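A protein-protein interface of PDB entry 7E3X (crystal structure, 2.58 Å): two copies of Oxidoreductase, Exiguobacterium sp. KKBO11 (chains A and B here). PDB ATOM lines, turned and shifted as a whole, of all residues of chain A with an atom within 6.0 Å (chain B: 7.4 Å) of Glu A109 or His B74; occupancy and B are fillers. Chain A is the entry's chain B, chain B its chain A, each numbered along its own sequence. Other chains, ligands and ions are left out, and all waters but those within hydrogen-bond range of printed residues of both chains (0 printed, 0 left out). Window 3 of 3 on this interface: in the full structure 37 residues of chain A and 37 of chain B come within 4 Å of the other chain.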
ATOM      1  N   GLU A 104      29.558  23.496   0.927  1.00  0.00           N
ATOM      2  CA  GLU A 104      28.487  24.466   1.087  1.00  0.00           C
ATOM      3  C   GLU A 104      28.279  25.130  -0.270  1.00  0.00           C
ATOM      4  O   GLU A 104      29.167  25.824  -0.772  1.00  0.00           O
ATOM      5  CB  GLU A 104      28.827  25.475   2.181  1.00  0.00           C
ATOM      6  CG  GLU A 104      27.669  26.394   2.552  1.00  0.00           C
ATOM      7  CD  GLU A 104      28.094  27.844   2.655  1.00  0.00           C
ATOM      8  OE1 GLU A 104      29.297  28.098   2.883  1.00  0.00           O
ATOM      9  OE2 GLU A 104      27.228  28.729   2.495  1.00  0.00           O
ATOM     10  N   LEU A 105      27.123  24.879  -0.885  1.00  0.00           N
ATOM     11  CA  LEU A 105      26.873  25.375  -2.234  1.00  0.00           C
ATOM     12  C   LEU A 105      27.137  26.873  -2.369  1.00  0.00           C
ATOM     13  O   LEU A 105      27.579  27.336  -3.424  1.00  0.00           O
ATOM     14  CB  LEU A 105      25.435  25.073  -2.627  1.00  0.00           C
ATOM     15  CG  LEU A 105      25.265  23.904  -3.579  1.00  0.00           C
ATOM     16  CD1 LEU A 105      26.047  24.196  -4.848  1.00  0.00           C
ATOM     17  CD2 LEU A 105      25.732  22.623  -2.925  1.00  0.00           C
ATOM     18  N   GLY A 106      26.869  27.649  -1.321  1.00  0.00           N
ATOM     19  CA  GLY A 106      27.063  29.083  -1.422  1.00  0.00           C
ATOM     20  C   GLY A 106      28.528  29.463  -1.436  1.00  0.00           C
ATOM     21  O   GLY A 106      28.943  30.332  -2.204  1.00  0.00           O
ATOM     22  N   LYS A 107      29.332  28.833  -0.579  1.00  0.00           N
ATOM     23  CA  LYS A 107      30.768  29.096  -0.628  1.00  0.00           C
ATOM     24  C   LYS A 107      31.352  28.701  -1.984  1.00  0.00           C
ATOM     25  O   LYS A 107      32.100  29.471  -2.599  1.00  0.00           O
ATOM     26  CB  LYS A 107      31.489  28.369   0.513  1.00  0.00           C
ATOM     27  CG  LYS A 107      32.954  28.781   0.703  1.00  0.00           C
ATOM     28  CD  LYS A 107      33.625  28.011   1.844  1.00  0.00           C
ATOM     29  CE  LYS A 107      35.127  28.166   1.830  1.00  0.00           C
ATOM     30  NZ  LYS A 107      35.747  27.102   2.662  1.00  0.00           N
ATOM     31  N   ILE A 108      30.987  27.525  -2.490  1.00  0.00           N
ATOM     32  CA  ILE A 108      31.531  27.096  -3.772  1.00  0.00           C
ATOM     33  C   ILE A 108      31.106  28.057  -4.864  1.00  0.00           C
ATOM     34  O   ILE A 108      31.914  28.442  -5.720  1.00  0.00           O
ATOM     35  CB  ILE A 108      31.113  25.648  -4.086  1.00  0.00           C
ATOM     36  CG1 ILE A 108      32.207  24.669  -3.630  1.00  0.00           C
ATOM     37  CG2 ILE A 108      30.864  25.472  -5.573  1.00  0.00           C
ATOM     38  CD1 ILE A 108      32.600  24.790  -2.154  1.00  0.00           C
ATOM     39  N   GLU A 109      29.848  28.492  -4.834  1.00  0.00           N
ATOM     40  CA  GLU A 109      29.365  29.424  -5.848  1.00  0.00           C
ATOM     41  C   GLU A 109      30.159  30.722  -5.815  1.00  0.00           C
ATOM     42  O   GLU A 109      30.582  31.234  -6.859  1.00  0.00           O
ATOM     43  CB  GLU A 109      27.884  29.695  -5.632  1.00  0.00           C
ATOM     44  CG  GLU A 109      26.995  28.621  -6.179  1.00  0.00           C
ATOM     45  CD  GLU A 109      25.558  28.811  -5.781  1.00  0.00           C
ATOM     46  OE1 GLU A 109      25.254  29.824  -5.131  1.00  0.00           O
ATOM     47  OE2 GLU A 109      24.737  27.942  -6.124  1.00  0.00           O
ATOM     48  N   LYS A 110      30.354  31.279  -4.617  1.00  0.00           N
ATOM     49  CA  LYS A 110      31.234  32.432  -4.475  1.00  0.00           C
ATOM     50  C   LYS A 110      32.596  32.141  -5.092  1.00  0.00           C
ATOM     51  O   LYS A 110      33.156  32.979  -5.807  1.00  0.00           O
ATOM     52  CB  LYS A 110      31.385  32.803  -2.998  1.00  0.00           C
ATOM     53  CG  LYS A 110      31.572  34.284  -2.708  1.00  0.00           C
ATOM     54  CD  LYS A 110      31.883  34.533  -1.215  1.00  0.00           C
ATOM     55  CE  LYS A 110      31.642  35.996  -0.799  1.00  0.00           C
ATOM     56  NZ  LYS A 110      31.662  36.171   0.697  1.00  0.00           N
ATOM     57  N   MET A 111      33.130  30.939  -4.854  1.00  0.00           N
ATOM     58  CA  MET A 111      34.448  30.595  -5.384  1.00  0.00           C
ATOM     59  C   MET A 111      34.453  30.651  -6.901  1.00  0.00           C
ATOM     60  O   MET A 111      35.327  31.287  -7.508  1.00  0.00           O
ATOM     61  CB  MET A 111      34.872  29.212  -4.907  1.00  0.00           C
ATOM     62  CG  MET A 111      36.331  28.931  -5.103  1.00  0.00           C
ATOM     63  SD  MET A 111      36.782  27.320  -4.461  1.00  0.00           S
ATOM     64  CE  MET A 111      35.653  26.238  -5.300  1.00  0.00           C
ATOM     65  N   LEU A 112      33.477  29.998  -7.535  1.00  0.00           N
ATOM     66  CA  LEU A 112      33.385  30.069  -8.987  1.00  0.00           C
ATOM     67  C   LEU A 112      33.373  31.514  -9.451  1.00  0.00           C
ATOM     68  O   LEU A 112      34.088  31.883 -10.394  1.00  0.00           O
ATOM     69  CB  LEU A 112      32.141  29.332  -9.483  1.00  0.00           C
ATOM     70  CG  LEU A 112      32.034  27.870  -9.078  1.00  0.00           C
ATOM     71  CD1 LEU A 112      30.825  27.226  -9.705  1.00  0.00           C
ATOM     72  CD2 LEU A 112      33.290  27.132  -9.481  1.00  0.00           C
ATOM     73  N   ARG A 113      32.589  32.357  -8.778  1.00  0.00           N
ATOM     74  CA  ARG A 113      32.420  33.730  -9.235  1.00  0.00           C
ATOM     75  C   ARG A 113      33.680  34.560  -9.056  1.00  0.00           C
ATOM     76  O   ARG A 113      33.971  35.430  -9.890  1.00  0.00           O
ATOM     77  CB  ARG A 113      31.246  34.356  -8.511  1.00  0.00           C
ATOM     78  CG  ARG A 113      29.962  33.679  -8.931  1.00  0.00           C
ATOM     79  CD  ARG A 113      28.813  34.559  -8.657  1.00  0.00           C
ATOM     80  NE  ARG A 113      28.802  34.843  -7.242  1.00  0.00           N
ATOM     81  CZ  ARG A 113      28.051  34.194  -6.366  1.00  0.00           C
ATOM     82  NH1 ARG A 113      27.227  33.229  -6.778  1.00  0.00           N
ATOM     83  NH2 ARG A 113      28.129  34.521  -5.081  1.00  0.00           N
ATOM     84  N   LEU A 114      34.448  34.299  -8.003  1.00  0.00           N
ATOM     85  CA  LEU A 114      35.728  34.976  -7.835  1.00  0.00           C
ATOM     86  C   LEU A 114      36.805  34.366  -8.739  1.00  0.00           C
ATOM     87  O   LEU A 114      37.392  35.050  -9.583  1.00  0.00           O
ATOM     88  CB  LEU A 114      36.134  34.909  -6.360  1.00  0.00           C
ATOM     89  CG  LEU A 114      37.402  35.639  -5.927  1.00  0.00           C
ATOM     90  CD1 LEU A 114      37.245  37.152  -6.031  1.00  0.00           C
ATOM     91  CD2 LEU A 114      37.779  35.227  -4.529  1.00  0.00           C
ATOM     92  N   VAL B  65      13.625  25.320 -18.422  1.00  0.00           N
ATOM     93  CA  VAL B  65      14.437  26.087 -17.482  1.00  0.00           C
ATOM     94  C   VAL B  65      15.601  26.721 -18.227  1.00  0.00           C
ATOM     95  O   VAL B  65      16.234  26.088 -19.081  1.00  0.00           O
ATOM     96  CB  VAL B  65      14.980  25.215 -16.329  1.00  0.00           C
ATOM     97  CG1 VAL B  65      15.535  26.083 -15.227  1.00  0.00           C
ATOM     98  CG2 VAL B  65      13.902  24.295 -15.802  1.00  0.00           C
ATOM     99  N   LEU B  67      19.143  27.493 -17.420  1.00  0.00           N
ATOM    100  CA  LEU B  67      20.113  27.059 -16.425  1.00  0.00           C
ATOM    101  C   LEU B  67      21.325  27.989 -16.329  1.00  0.00           C
ATOM    102  O   LEU B  67      22.260  27.692 -15.580  1.00  0.00           O
ATOM    103  CB  LEU B  67      20.568  25.628 -16.730  1.00  0.00           C
ATOM    104  CG  LEU B  67      19.548  24.490 -16.586  1.00  0.00           C
ATOM    105  CD1 LEU B  67      20.079  23.188 -17.201  1.00  0.00           C
ATOM    106  CD2 LEU B  67      19.200  24.279 -15.133  1.00  0.00           C
ATOM    107  N   ASP B  69      20.935  30.704 -14.930  1.00  0.00           N
ATOM    108  CA  ASP B  69      20.571  31.399 -13.704  1.00  0.00           C
ATOM    109  C   ASP B  69      20.725  30.440 -12.529  1.00  0.00           C
ATOM    110  O   ASP B  69      20.130  29.357 -12.529  1.00  0.00           O
ATOM    111  CB  ASP B  69      19.140  31.937 -13.783  1.00  0.00           C
ATOM    112  CG  ASP B  69      18.631  32.444 -12.440  1.00  0.00           C
ATOM    113  OD1 ASP B  69      18.942  33.594 -12.047  1.00  0.00           O
ATOM    114  OD2 ASP B  69      17.928  31.663 -11.765  1.00  0.00           O
ATOM    115  N   ASN B  70      21.517  30.851 -11.523  1.00  0.00           N
ATOM    116  CA  ASN B  70      21.886  29.945 -10.429  1.00  0.00           C
ATOM    117  C   ASN B  70      20.688  29.588  -9.565  1.00  0.00           C
ATOM    118  O   ASN B  70      20.604  28.467  -9.046  1.00  0.00           O
ATOM    119  CB  ASN B  70      22.987  30.557  -9.565  1.00  0.00           C
ATOM    120  CG  ASN B  70      24.380  30.487 -10.235  1.00  0.00           C
ATOM    121  OD1 ASN B  70      24.563  29.861 -11.286  1.00  0.00           O
ATOM    122  ND2 ASN B  70      25.360  31.136  -9.615  1.00  0.00           N
ATOM    123  N   GLN B  71      19.755  30.529  -9.384  1.00  0.00           N
ATOM    124  CA  GLN B  71      18.545  30.201  -8.647  1.00  0.00           C
ATOM    125  C   GLN B  71      17.664  29.245  -9.445  1.00  0.00           C
ATOM    126  O   GLN B  71      17.013  28.370  -8.860  1.00  0.00           O
ATOM    127  CB  GLN B  71      17.801  31.484  -8.265  1.00  0.00           C
ATOM    128  CG  GLN B  71      16.733  31.303  -7.171  1.00  0.00           C
ATOM    129  CD  GLN B  71      17.208  30.493  -5.954  1.00  0.00           C
ATOM    130  OE1 GLN B  71      18.371  30.574  -5.532  1.00  0.00           O
ATOM    131  NE2 GLN B  71      16.297  29.690  -5.398  1.00  0.00           N
ATOM    132  N   ASN B  72      17.655  29.378 -10.777  1.00  0.00           N
ATOM    133  CA  ASN B  72      16.929  28.428 -11.617  1.00  0.00           C
ATOM    134  C   ASN B  72      17.460  27.014 -11.428  1.00  0.00           C
ATOM    135  O   ASN B  72      16.686  26.050 -11.360  1.00  0.00           O
ATOM    136  CB  ASN B  72      17.055  28.828 -13.082  1.00  0.00           C
ATOM    137  CG  ASN B  72      15.978  29.767 -13.519  1.00  0.00           C
ATOM    138  OD1 ASN B  72      15.149  30.198 -12.718  1.00  0.00           O
ATOM    139  ND2 ASN B  72      15.982  30.103 -14.799  1.00  0.00           N
ATOM    140  N   VAL B  73      18.785  26.879 -11.352  1.00  0.00           N
ATOM    141  CA  VAL B  73      19.415  25.572 -11.188  1.00  0.00           C
ATOM    142  C   VAL B  73      18.994  24.945  -9.863  1.00  0.00           C
ATOM    143  O   VAL B  73      18.581  23.780  -9.806  1.00  0.00           O
ATOM    144  CB  VAL B  73      20.948  25.713 -11.299  1.00  0.00           C
ATOM    145  CG1 VAL B  73      21.630  24.408 -10.949  1.00  0.00           C
ATOM    146  CG2 VAL B  73      21.355  26.208 -12.710  1.00  0.00           C
ATOM    147  N   HIS B  74      19.086  25.715  -8.781  1.00  0.00           N
ATOM    148  CA  HIS B  74      18.662  25.230  -7.478  1.00  0.00           C
ATOM    149  C   HIS B  74      17.199  24.793  -7.500  1.00  0.00           C
ATOM    150  O   HIS B  74      16.856  23.691  -7.044  1.00  0.00           O
ATOM    151  CB  HIS B  74      18.866  26.329  -6.452  1.00  0.00           C
ATOM    152  CG  HIS B  74      20.276  26.480  -5.987  1.00  0.00           C
ATOM    153  ND1 HIS B  74      20.825  25.683  -5.002  1.00  0.00           N
ATOM    154  CD2 HIS B  74      21.240  27.360  -6.345  1.00  0.00           C
ATOM    155  CE1 HIS B  74      22.070  26.064  -4.777  1.00  0.00           C
ATOM    156  NE2 HIS B  74      22.346  27.079  -5.580  1.00  0.00           N
ATOM    157  N   ASP B  75      16.315  25.654  -8.018  1.00  0.00           N
ATOM    158  CA  ASP B  75      14.894  25.326  -8.067  1.00  0.00           C
ATOM    159  C   ASP B  75      14.669  24.013  -8.801  1.00  0.00           C
ATOM    160  O   ASP B  75      13.920  23.151  -8.331  1.00  0.00           O
ATOM    161  CB  ASP B  75      14.114  26.458  -8.737  1.00  0.00           C
ATOM    162  CG  ASP B  75      14.129  27.744  -7.929  1.00  0.00           C
ATOM    163  OD1 ASP B  75      14.532  27.726  -6.748  1.00  0.00           O
ATOM    164  OD2 ASP B  75      13.736  28.788  -8.486  1.00  0.00           O
ATOM    165  N   LEU B  76      15.348  23.833  -9.943  1.00  0.00           N
ATOM    166  CA  LEU B  76      15.230  22.607 -10.734  1.00  0.00           C
ATOM    167  C   LEU B  76      15.520  21.360  -9.902  1.00  0.00           C
ATOM    168  O   LEU B  76      14.722  20.415  -9.875  1.00  0.00           O
ATOM    169  CB  LEU B  76      16.175  22.645 -11.935  1.00  0.00           C
ATOM    170  CG  LEU B  76      16.239  21.268 -12.622  1.00  0.00           C
ATOM    171  CD1 LEU B  76      14.932  20.953 -13.363  1.00  0.00           C
ATOM    172  CD2 LEU B  76      17.446  21.143 -13.554  1.00  0.00           C
ATOM    173  N   TYR B  77      16.676  21.327  -9.236  1.00  0.00           N
ATOM    174  CA  TYR B  77      17.012  20.158  -8.435  1.00  0.00           C
ATOM    175  C   TYR B  77      15.978  19.938  -7.350  1.00  0.00           C
ATOM    176  O   TYR B  77      15.546  18.807  -7.116  1.00  0.00           O
ATOM    177  CB  TYR B  77      18.392  20.302  -7.805  1.00  0.00           C
ATOM    178  CG  TYR B  77      18.842  19.034  -7.125  1.00  0.00           C
ATOM    179  CD1 TYR B  77      19.376  17.980  -7.867  1.00  0.00           C
ATOM    180  CD2 TYR B  77      18.711  18.874  -5.756  1.00  0.00           C
ATOM    181  CE1 TYR B  77      19.779  16.811  -7.262  1.00  0.00           C
ATOM    182  CE2 TYR B  77      19.103  17.709  -5.140  1.00  0.00           C
ATOM    183  CZ  TYR B  77      19.640  16.674  -5.899  1.00  0.00           C
ATOM    184  OH  TYR B  77      20.043  15.493  -5.296  1.00  0.00           O
ATOM    185  N   GLU B  78      15.573  21.013  -6.672  1.00  0.00           N
ATOM    186  CA  GLU B  78      14.659  20.870  -5.546  1.00  0.00           C
ATOM    187  C   GLU B  78      13.307  20.328  -5.992  1.00  0.00           C
ATOM    188  O   GLU B  78      12.638  19.618  -5.231  1.00  0.00           O
ATOM    189  CB  GLU B  78      14.502  22.215  -4.839  1.00  0.00           C
ATOM    190  CG  GLU B  78      13.411  22.274  -3.787  1.00  0.00           C
ATOM    191  CD  GLU B  78      13.816  21.641  -2.463  1.00  0.00           C
ATOM    192  OE1 GLU B  78      14.958  21.138  -2.366  1.00  0.00           O
ATOM    193  OE2 GLU B  78      12.995  21.661  -1.512  1.00  0.00           O
ATOM    194  N   GLY B  79      12.904  20.630  -7.230  1.00  0.00           N
ATOM    195  CA  GLY B  79      11.654  20.119  -7.766  1.00  0.00           C
ATOM    196  C   GLY B  79      11.686  18.647  -8.130  1.00  0.00           C
ATOM    197  O   GLY B  79      10.623  18.041  -8.282  1.00  0.00           O
ATOM    198  N   LEU B  80      12.879  18.059  -8.261  1.00  0.00           N
ATOM    199  CA  LEU B  80      13.062  16.656  -8.628  1.00  0.00           C
ATOM    200  C   LEU B  80      13.539  15.792  -7.466  1.00  0.00           C
ATOM    201  O   LEU B  80      13.823  14.604  -7.665  1.00  0.00           O
ATOM    202  CB  LEU B  80      14.066  16.527  -9.776  1.00  0.00           C
ATOM    203  CG  LEU B  80      13.870  17.441 -10.964  1.00  0.00           C
ATOM    204  CD1 LEU B  80      15.051  17.308 -11.901  1.00  0.00           C
ATOM    205  CD2 LEU B  80      12.590  17.060 -11.653  1.00  0.00           C
ATOM    206  N   LYS B  81      13.639  16.371  -6.265  1.00  0.00           N
ATOM    207  CA  LYS B  81      14.103  15.625  -5.058  1.00  0.00           C
ATOM    208  C   LYS B  81      13.077  14.553  -4.668  1.00  0.00           C
ATOM    209  O   LYS B  81      13.421  13.671  -3.869  1.00  0.00           O
ATOM    210  CB  LYS B  81      14.325  16.568  -3.872  1.00  0.00           C
ATOM    211  CG  LYS B  81      15.620  17.365  -3.890  1.00  0.00           C
ATOM    212  CD  LYS B  81      15.804  18.241  -2.671  1.00  0.00           C
ATOM    213  CE  LYS B  81      16.690  17.627  -1.609  1.00  0.00           C
ATOM    214  NZ  LYS B  81      16.312  16.231  -1.293  1.00  0.00           N
ATOM    215  N   GLU B 117      28.905  26.658 -13.771  1.00  0.00           N
ATOM    216  CA  GLU B 117      28.224  26.790 -12.494  1.00  0.00           C
ATOM    217  C   GLU B 117      27.062  25.818 -12.390  1.00  0.00           C
ATOM    218  O   GLU B 117      26.978  25.035 -11.438  1.00  0.00           O
ATOM    219  CB  GLU B 117      27.746  28.215 -12.325  1.00  0.00           C
ATOM    220  CG  GLU B 117      28.870  29.145 -12.110  1.00  0.00           C
ATOM    221  CD  GLU B 117      28.402  30.510 -11.710  1.00  0.00           C
ATOM    222  OE1 GLU B 117      27.181  30.718 -11.539  1.00  0.00           O
ATOM    223  OE2 GLU B 117      29.276  31.367 -11.530  1.00  0.00           O
ATOM    224  N   THR B 120      28.239  22.447 -11.936  1.00  0.00           N
ATOM    225  CA  THR B 120      28.816  22.214 -10.620  1.00  0.00           C
ATOM    226  C   THR B 120      27.728  22.139  -9.560  1.00  0.00           C
ATOM    227  O   THR B 120      27.745  21.235  -8.712  1.00  0.00           O
ATOM    228  CB  THR B 120      29.831  23.309 -10.294  1.00  0.00           C
ATOM    229  OG1 THR B 120      30.912  23.258 -11.234  1.00  0.00           O
ATOM    230  CG2 THR B 120      30.392  23.126  -8.903  1.00  0.00           C
ATOM    231  N   ILE B 121      26.751  23.051  -9.614  1.00  0.00           N
ATOM    232  CA  ILE B 121      25.650  23.007  -8.655  1.00  0.00           C
ATOM    233  C   ILE B 121      24.906  21.679  -8.756  1.00  0.00           C
ATOM    234  O   ILE B 121      24.683  20.993  -7.748  1.00  0.00           O
ATOM    235  CB  ILE B 121      24.703  24.200  -8.852  1.00  0.00           C
ATOM    236  CG1 ILE B 121      25.424  25.509  -8.547  1.00  0.00           C
ATOM    237  CG2 ILE B 121      23.518  24.060  -7.915  1.00  0.00           C
ATOM    238  CD1 ILE B 121      24.889  26.703  -9.315  1.00  0.00           C
ATOM    239  N   LEU B 122      24.513  21.288  -9.968  1.00  0.00           N
ATOM    240  CA  LEU B 122      23.734  20.061 -10.087  1.00  0.00           C
ATOM    241  C   LEU B 122      24.586  18.842  -9.746  1.00  0.00           C
ATOM    242  O   LEU B 122      24.107  17.926  -9.065  1.00  0.00           O
ATOM    243  CB  LEU B 122      23.125  19.952 -11.487  1.00  0.00           C
ATOM    244  CG  LEU B 122      22.152  21.070 -11.892  1.00  0.00           C
ATOM    245  CD1 LEU B 122      21.814  21.024 -13.379  1.00  0.00           C
ATOM    246  CD2 LEU B 122      20.872  21.046 -11.046  1.00  0.00           C
ATOM    247  N   LEU B 125      24.758  18.778  -5.713  1.00  0.00           N
ATOM    248  CA  LEU B 125      23.553  18.315  -5.029  1.00  0.00           C
ATOM    249  C   LEU B 125      23.324  16.830  -5.281  1.00  0.00           C
ATOM    250  O   LEU B 125      22.990  16.078  -4.358  1.00  0.00           O
ATOM    251  CB  LEU B 125      22.347  19.133  -5.484  1.00  0.00           C
ATOM    252  CG  LEU B 125      22.450  20.620  -5.157  1.00  0.00           C
ATOM    253  CD1 LEU B 125      21.574  21.449  -6.088  1.00  0.00           C
ATOM    254  CD2 LEU B 125      22.080  20.840  -3.710  1.00  0.00           C
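The side-chain amide nitrogen of Asn B70 is in hydrogen-bond range of the side-chain carboxylate of Glu B117 (2.7 Å).
Glu A109 touches just these residues of chain B: His B74 and Ile B121.
His B74 touches just one residue of chain A: Glu A109.
Of the printed residues of chain B, Arg A113 touches Asn B70 and Glu B117.
Printed residues of chain A within 4 Å of Ile B121: Leu A105 (3.97 Å) and Glu A109 (3.4 Å).
Of the printed residues of chain A, Asn B70 touches Arg A113.
Leu B67 touches none of the printed residues of chain A.
The nearest residue of chain B that does not touch Glu A109 is Asn B70 (4.5 Å).
The nearest printed residue of chain A that does not touch Ile B121 is Leu A112 (5.8 Å).
CD1 of Leu A105 touches CG1 of Ile B121, at 3.97 Å.
OE2 of Glu A109 touches CD1 of Ile B121 (3.4 Å).
Glu B117 touches Leu A112 (CG to CD1, 3.6 Å).
Arg A113 touches Asn B70 (NH1 to ND2, 3.99 Å).
Arg A113 touches Glu B117 (CG to OE2, 3.5 Å).
No position is printed for both chains.
A ring nitrogen (NE2) of His B74 is in hydrogen-bond range of the side-chain carboxylate of Glu A109, at 2.6 Å.
Printed residues of chain B that touch a printed residue of chain A: Asn B70, His B74, Glu B117 and Ile B121.
Hydrophobic or aromatic side chains of chain A within 4 Å of the printed part of chain B: Leu A105 and Leu A112.
Among the printed residues, no Asp or Glu carboxylate lies within 4 Å of a Lys or Arg side-chain nitrogen of the other chain.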
